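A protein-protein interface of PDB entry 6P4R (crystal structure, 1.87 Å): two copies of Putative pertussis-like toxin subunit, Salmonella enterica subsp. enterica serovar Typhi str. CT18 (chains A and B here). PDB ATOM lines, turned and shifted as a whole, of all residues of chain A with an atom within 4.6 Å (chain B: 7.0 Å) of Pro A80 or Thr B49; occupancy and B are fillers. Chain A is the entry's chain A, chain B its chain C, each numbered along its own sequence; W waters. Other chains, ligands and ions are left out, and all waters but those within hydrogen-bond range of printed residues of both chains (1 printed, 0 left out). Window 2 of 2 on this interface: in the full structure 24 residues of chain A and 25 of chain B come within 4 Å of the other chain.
NE2 of Gln B46 sits at hydrogen-bond distance from OE2 of Glu A24 (2.8 Å). O of Glu A24 lies within hydrogen-bond range of N of Asp B48 (3.0 Å). The side-chain carboxylate (OE2) of Glu A24 is in hydrogen-bond range of the backbone NH (N) of Thr B49, 2.6 Å away. The backbone carbonyl oxygen (O) of Ile A77 sits at hydrogen-bond distance from the side-chain amide nitrogen (NE2) of Gln B46 (2.7 Å). OE1 of Gln B46 lies close to O of Trp A78 (3.3 Å). OG of Ser A81 lies within hydrogen-bond range of OE1 of Gln B46, 2.7 Å away.
N of Trp A78 lies close to OG of Ser A76, 3.2 Å away. OG1 of Thr B49 lies close to NZ of Lys B74 (3.1 Å). The backbone carbonyl oxygen of Pro B51 lies within hydrogen-bond range of the backbone NH of Ser B73 (2.8 Å).
Among the printed residues, merely in contact across the chains: Glu A24 with Ile B47, Pro A80 with Gln B46, Pro A80 with Thr B49, Pro A80 with Pro B51 and Ser A81 with Pro B51.
Pro A80 touches three residues of chain B. Printed residues of chain B within 4 Å of Ser A81: Gln B46 (2.7 Å) and Pro B51 (3.5 Å). Of the printed residues of chain A, Gln B46 touches Glu A24, Ile A77, Trp A78, Pro A80 and Ser A81. Of the printed residues of chain A, Asp B48 touches Glu A24. Thr B49 touches just these residues of chain A: Glu A24 and Pro A80. Printed residues of chain A within 4 Å of Pro B51: Pro A80 and Ser A81. Lys B74 touches none of the printed residues of chain A. Gln B75 touches none of the printed residues of chain A. The nearest residue of chain B that does not touch Pro A80 is Ser B50 (5.5 Å).
Of the 8 printed residues of chain A, 5 touch a printed residue of chain B. Along chain A the printed residues that touch a printed residue of chain B span positions 24 to 81. Of the 9 printed residues of chain B, 5 touch a printed residue of chain A. Printed residues of chain B that touch a printed residue of chain A: Gln B46, Ile B47, Asp B48, Thr B49 and Pro B51. Among the printed residues, no Asp or Glu carboxylate lies within 4 Å of a Lys or Arg side-chain nitrogen of the other chain.
No position is printed for both chains.
Water W1 lies within hydrogen-bond range of OD1 of Asp B48 and N of Glu A24.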
ATOM      1  N   GLU A  24      16.019 -34.771 -19.808  1.00  0.00           N
ATOM      2  CA  GLU A  24      15.387 -34.719 -21.123  1.00  0.00           C
ATOM      3  C   GLU A  24      16.406 -35.111 -22.186  1.00  0.00           C
ATOM      4  O   GLU A  24      17.617 -34.954 -21.996  1.00  0.00           O
ATOM      5  CB  GLU A  24      14.819 -33.319 -21.404  1.00  0.00           C
ATOM      6  CG  GLU A  24      15.748 -32.373 -22.165  1.00  0.00           C
ATOM      7  CD  GLU A  24      17.004 -31.952 -21.392  1.00  0.00           C
ATOM      8  OE1 GLU A  24      17.163 -32.335 -20.219  1.00  0.00           O
ATOM      9  OE2 GLU A  24      17.862 -31.250 -21.984  1.00  0.00           O
ATOM     10  N   SER A  76      11.667 -22.653 -22.811  1.00  0.00           N
ATOM     11  CA  SER A  76      11.596 -24.099 -22.623  1.00  0.00           C
ATOM     12  C   SER A  76      12.973 -24.712 -22.376  1.00  0.00           C
ATOM     13  O   SER A  76      14.007 -24.066 -22.576  1.00  0.00           O
ATOM     14  CB  SER A  76      10.920 -24.791 -23.822  1.00  0.00           C
ATOM     15  OG  SER A  76      11.881 -25.133 -24.818  1.00  0.00           O
ATOM     16  N   ILE A  77      12.980 -25.957 -21.894  1.00  0.00           N
ATOM     17  CA  ILE A  77      14.226 -26.643 -21.571  1.00  0.00           C
ATOM     18  C   ILE A  77      15.096 -26.808 -22.807  1.00  0.00           C
ATOM     19  O   ILE A  77      16.303 -26.965 -22.681  1.00  0.00           O
ATOM     20  CB  ILE A  77      13.922 -28.008 -20.894  1.00  0.00           C
ATOM     21  CG1 ILE A  77      15.197 -28.648 -20.348  1.00  0.00           C
ATOM     22  CG2 ILE A  77      13.190 -28.948 -21.851  1.00  0.00           C
ATOM     23  CD1 ILE A  77      14.941 -29.691 -19.278  1.00  0.00           C
ATOM     24  N   TRP A  78      14.512 -26.714 -24.012  1.00  0.00           N
ATOM     25  CA  TRP A  78      15.256 -26.852 -25.264  1.00  0.00           C
ATOM     26  C   TRP A  78      15.943 -25.566 -25.720  1.00  0.00           C
ATOM     27  O   TRP A  78      16.659 -25.590 -26.733  1.00  0.00           O
ATOM     28  CB  TRP A  78      14.318 -27.331 -26.376  1.00  0.00           C
ATOM     29  CG  TRP A  78      13.540 -28.563 -25.978  1.00  0.00           C
ATOM     30  CD1 TRP A  78      12.225 -28.624 -25.643  1.00  0.00           C
ATOM     31  CD2 TRP A  78      14.047 -29.901 -25.872  1.00  0.00           C
ATOM     32  NE1 TRP A  78      11.866 -29.920 -25.334  1.00  0.00           N
ATOM     33  CE2 TRP A  78      12.971 -30.723 -25.460  1.00  0.00           C
ATOM     34  CE3 TRP A  78      15.304 -30.484 -26.086  1.00  0.00           C
ATOM     35  CZ2 TRP A  78      13.110 -32.089 -25.269  1.00  0.00           C
ATOM     36  CZ3 TRP A  78      15.446 -31.846 -25.892  1.00  0.00           C
ATOM     37  CH2 TRP A  78      14.351 -32.638 -25.487  1.00  0.00           C
ATOM     38  N   ALA A  79      15.727 -24.453 -25.014  1.00  0.00           N
ATOM     39  CA  ALA A  79      16.330 -23.174 -25.393  1.00  0.00           C
ATOM     40  C   ALA A  79      17.829 -23.224 -25.677  1.00  0.00           C
ATOM     41  O   ALA A  79      18.260 -22.570 -26.645  1.00  0.00           O
ATOM     42  CB  ALA A  79      16.047 -22.137 -24.296  1.00  0.00           C
ATOM     43  N   PRO A  80      18.659 -23.949 -24.921  1.00  0.00           N
ATOM     44  CA  PRO A  80      20.101 -23.937 -25.221  1.00  0.00           C
ATOM     45  C   PRO A  80      20.442 -24.378 -26.637  1.00  0.00           C
ATOM     46  O   PRO A  80      21.463 -23.939 -27.173  1.00  0.00           O
ATOM     47  CB  PRO A  80      20.680 -24.913 -24.185  1.00  0.00           C
ATOM     48  CG  PRO A  80      19.736 -24.873 -23.064  1.00  0.00           C
ATOM     49  CD  PRO A  80      18.375 -24.696 -23.675  1.00  0.00           C
ATOM     50  N   SER A  81      19.615 -25.210 -27.259  1.00  0.00           N
ATOM     51  CA  SER A  81      19.920 -25.775 -28.570  1.00  0.00           C
ATOM     52  C   SER A  81      19.398 -24.927 -29.721  1.00  0.00           C
ATOM     53  O   SER A  81      19.493 -25.360 -30.879  1.00  0.00           O
ATOM     54  CB  SER A  81      19.347 -27.192 -28.670  1.00  0.00           C
ATOM     55  OG  SER A  81      20.023 -28.032 -27.764  1.00  0.00           O
ATOM     56  N   PHE A  82      18.869 -23.727 -29.437  1.00  0.00           N
ATOM     57  CA  PHE A  82      18.215 -22.932 -30.478  1.00  0.00           C
ATOM     58  C   PHE A  82      19.153 -22.669 -31.654  1.00  0.00           C
ATOM     59  O   PHE A  82      18.788 -22.900 -32.811  1.00  0.00           O
ATOM     60  CB  PHE A  82      17.699 -21.609 -29.900  1.00  0.00           C
ATOM     61  CG  PHE A  82      17.168 -20.659 -30.944  1.00  0.00           C
ATOM     62  CD1 PHE A  82      15.854 -20.773 -31.403  1.00  0.00           C
ATOM     63  CD2 PHE A  82      17.980 -19.660 -31.473  1.00  0.00           C
ATOM     64  CE1 PHE A  82      15.360 -19.897 -32.391  1.00  0.00           C
ATOM     65  CE2 PHE A  82      17.501 -18.789 -32.461  1.00  0.00           C
ATOM     66  CZ  PHE A  82      16.184 -18.905 -32.909  1.00  0.00           C
ATOM     67  N   GLN B  46      19.739 -32.472 -28.067  1.00  0.00           N
ATOM     68  CA  GLN B  46      20.020 -31.962 -26.723  1.00  0.00           C
ATOM     69  C   GLN B  46      19.839 -33.094 -25.726  1.00  0.00           C
ATOM     70  O   GLN B  46      18.948 -33.932 -25.887  1.00  0.00           O
ATOM     71  CB  GLN B  46      19.089 -30.795 -26.354  1.00  0.00           C
ATOM     72  CG  GLN B  46      19.436 -30.149 -25.019  1.00  0.00           C
ATOM     73  CD  GLN B  46      18.628 -28.908 -24.724  1.00  0.00           C
ATOM     74  OE1 GLN B  46      18.680 -27.926 -25.465  1.00  0.00           O
ATOM     75  NE2 GLN B  46      17.875 -28.944 -23.635  1.00  0.00           N
ATOM     76  N   ILE B  47      20.666 -33.104 -24.678  1.00  0.00           N
ATOM     77  CA  ILE B  47      20.507 -34.057 -23.573  1.00  0.00           C
ATOM     78  C   ILE B  47      20.929 -33.389 -22.269  1.00  0.00           C
ATOM     79  O   ILE B  47      21.995 -32.774 -22.191  1.00  0.00           O
ATOM     80  CB  ILE B  47      21.300 -35.362 -23.803  1.00  0.00           C
ATOM     81  CG1 ILE B  47      20.986 -36.371 -22.685  1.00  0.00           C
ATOM     82  CG2 ILE B  47      22.809 -35.087 -23.933  1.00  0.00           C
ATOM     83  CD1 ILE B  47      21.336 -37.824 -23.027  1.00  0.00           C
ATOM     84  N   ASP B  48      20.075 -33.496 -21.245  1.00  0.00           N
ATOM     85  CA  ASP B  48      20.392 -32.998 -19.902  1.00  0.00           C
ATOM     86  C   ASP B  48      20.859 -31.541 -19.937  1.00  0.00           C
ATOM     87  O   ASP B  48      21.860 -31.170 -19.312  1.00  0.00           O
ATOM     88  CB  ASP B  48      21.443 -33.887 -19.231  1.00  0.00           C
ATOM     89  CG  ASP B  48      20.894 -35.229 -18.835  1.00  0.00           C
ATOM     90  OD1 ASP B  48      19.704 -35.288 -18.428  1.00  0.00           O
ATOM     91  OD2 ASP B  48      21.647 -36.229 -18.937  1.00  0.00           O
ATOM     92  N   THR B  49      20.104 -30.715 -20.679  1.00  0.00           N
ATOM     93  CA  THR B  49      20.286 -29.275 -20.926  1.00  0.00           C
ATOM     94  C   THR B  49      21.472 -28.951 -21.818  1.00  0.00           C
ATOM     95  O   THR B  49      21.757 -27.762 -22.052  1.00  0.00           O
ATOM     96  CB  THR B  49      20.399 -28.428 -19.642  1.00  0.00           C
ATOM     97  OG1 THR B  49      21.699 -28.590 -19.042  1.00  0.00           O
ATOM     98  CG2 THR B  49      19.323 -28.821 -18.666  1.00  0.00           C
ATOM     99  N   SER B  50      22.151 -29.951 -22.365  1.00  0.00           N
ATOM    100  CA  SER B  50      23.326 -29.667 -23.167  1.00  0.00           C
ATOM    101  C   SER B  50      23.062 -29.971 -24.634  1.00  0.00           C
ATOM    102  O   SER B  50      22.722 -31.116 -24.974  1.00  0.00           O
ATOM    103  CB  SER B  50      24.524 -30.474 -22.675  1.00  0.00           C
ATOM    104  OG  SER B  50      25.602 -30.270 -23.577  1.00  0.00           O
ATOM    105  N   PRO B  51      23.233 -28.995 -25.526  1.00  0.00           N
ATOM    106  CA  PRO B  51      23.301 -29.303 -26.958  1.00  0.00           C
ATOM    107  C   PRO B  51      24.368 -30.351 -27.228  1.00  0.00           C
ATOM    108  O   PRO B  51      25.421 -30.365 -26.585  1.00  0.00           O
ATOM    109  CB  PRO B  51      23.683 -27.960 -27.583  1.00  0.00           C
ATOM    110  CG  PRO B  51      23.194 -26.944 -26.600  1.00  0.00           C
ATOM    111  CD  PRO B  51      23.404 -27.555 -25.261  1.00  0.00           C
ATOM    112  N   SER B  73      27.948 -30.443 -25.318  1.00  0.00           N
ATOM    113  CA  SER B  73      28.419 -29.065 -25.162  1.00  0.00           C
ATOM    114  C   SER B  73      29.008 -28.771 -23.786  1.00  0.00           C
ATOM    115  O   SER B  73      29.964 -27.992 -23.675  1.00  0.00           O
ATOM    116  CB  SER B  73      27.283 -28.082 -25.438  1.00  0.00           C
ATOM    117  OG  SER B  73      27.846 -26.788 -25.597  1.00  0.00           O
ATOM    118  N   LYS B  74      28.441 -29.317 -22.720  1.00  0.00           N
ATOM    119  CA  LYS B  74      29.041 -28.942 -21.438  1.00  0.00           C
ATOM    120  C   LYS B  74      29.442 -30.155 -20.612  1.00  0.00           C
ATOM    121  O   LYS B  74      29.439 -30.099 -19.372  1.00  0.00           O
ATOM    122  CB  LYS B  74      28.113 -28.030 -20.639  1.00  0.00           C
ATOM    123  CG  LYS B  74      26.673 -28.441 -20.664  1.00  0.00           C
ATOM    124  CD  LYS B  74      25.756 -27.252 -20.308  1.00  0.00           C
ATOM    125  CE  LYS B  74      24.567 -27.712 -19.489  1.00  0.00           C
ATOM    126  NZ  LYS B  74      24.132 -26.742 -18.418  1.00  0.00           N
ATOM    127  N   GLN B  75      29.821 -31.254 -21.266  1.00  0.00           N
ATOM    128  CA  GLN B  75      30.233 -32.451 -20.562  1.00  0.00           C
ATOM    129  C   GLN B  75      31.525 -33.006 -21.155  1.00  0.00           C
ATOM    130  O   GLN B  75      31.803 -32.838 -22.351  1.00  0.00           O
ATOM    131  CB  GLN B  75      29.121 -33.527 -20.566  1.00  0.00           C
ATOM    132  CG  GLN B  75      27.812 -33.077 -19.914  1.00  0.00           C
ATOM    133  CD  GLN B  75      27.900 -33.108 -18.358  1.00  0.00           C
ATOM    134  OE1 GLN B  75      27.265 -32.301 -17.663  1.00  0.00           O
ATOM    135  NE2 GLN B  75      28.702 -34.037 -17.824  1.00  0.00           N
HETATM  136  O   HOH W   1      17.850 -37.167 -19.055  1.00  0.00           O
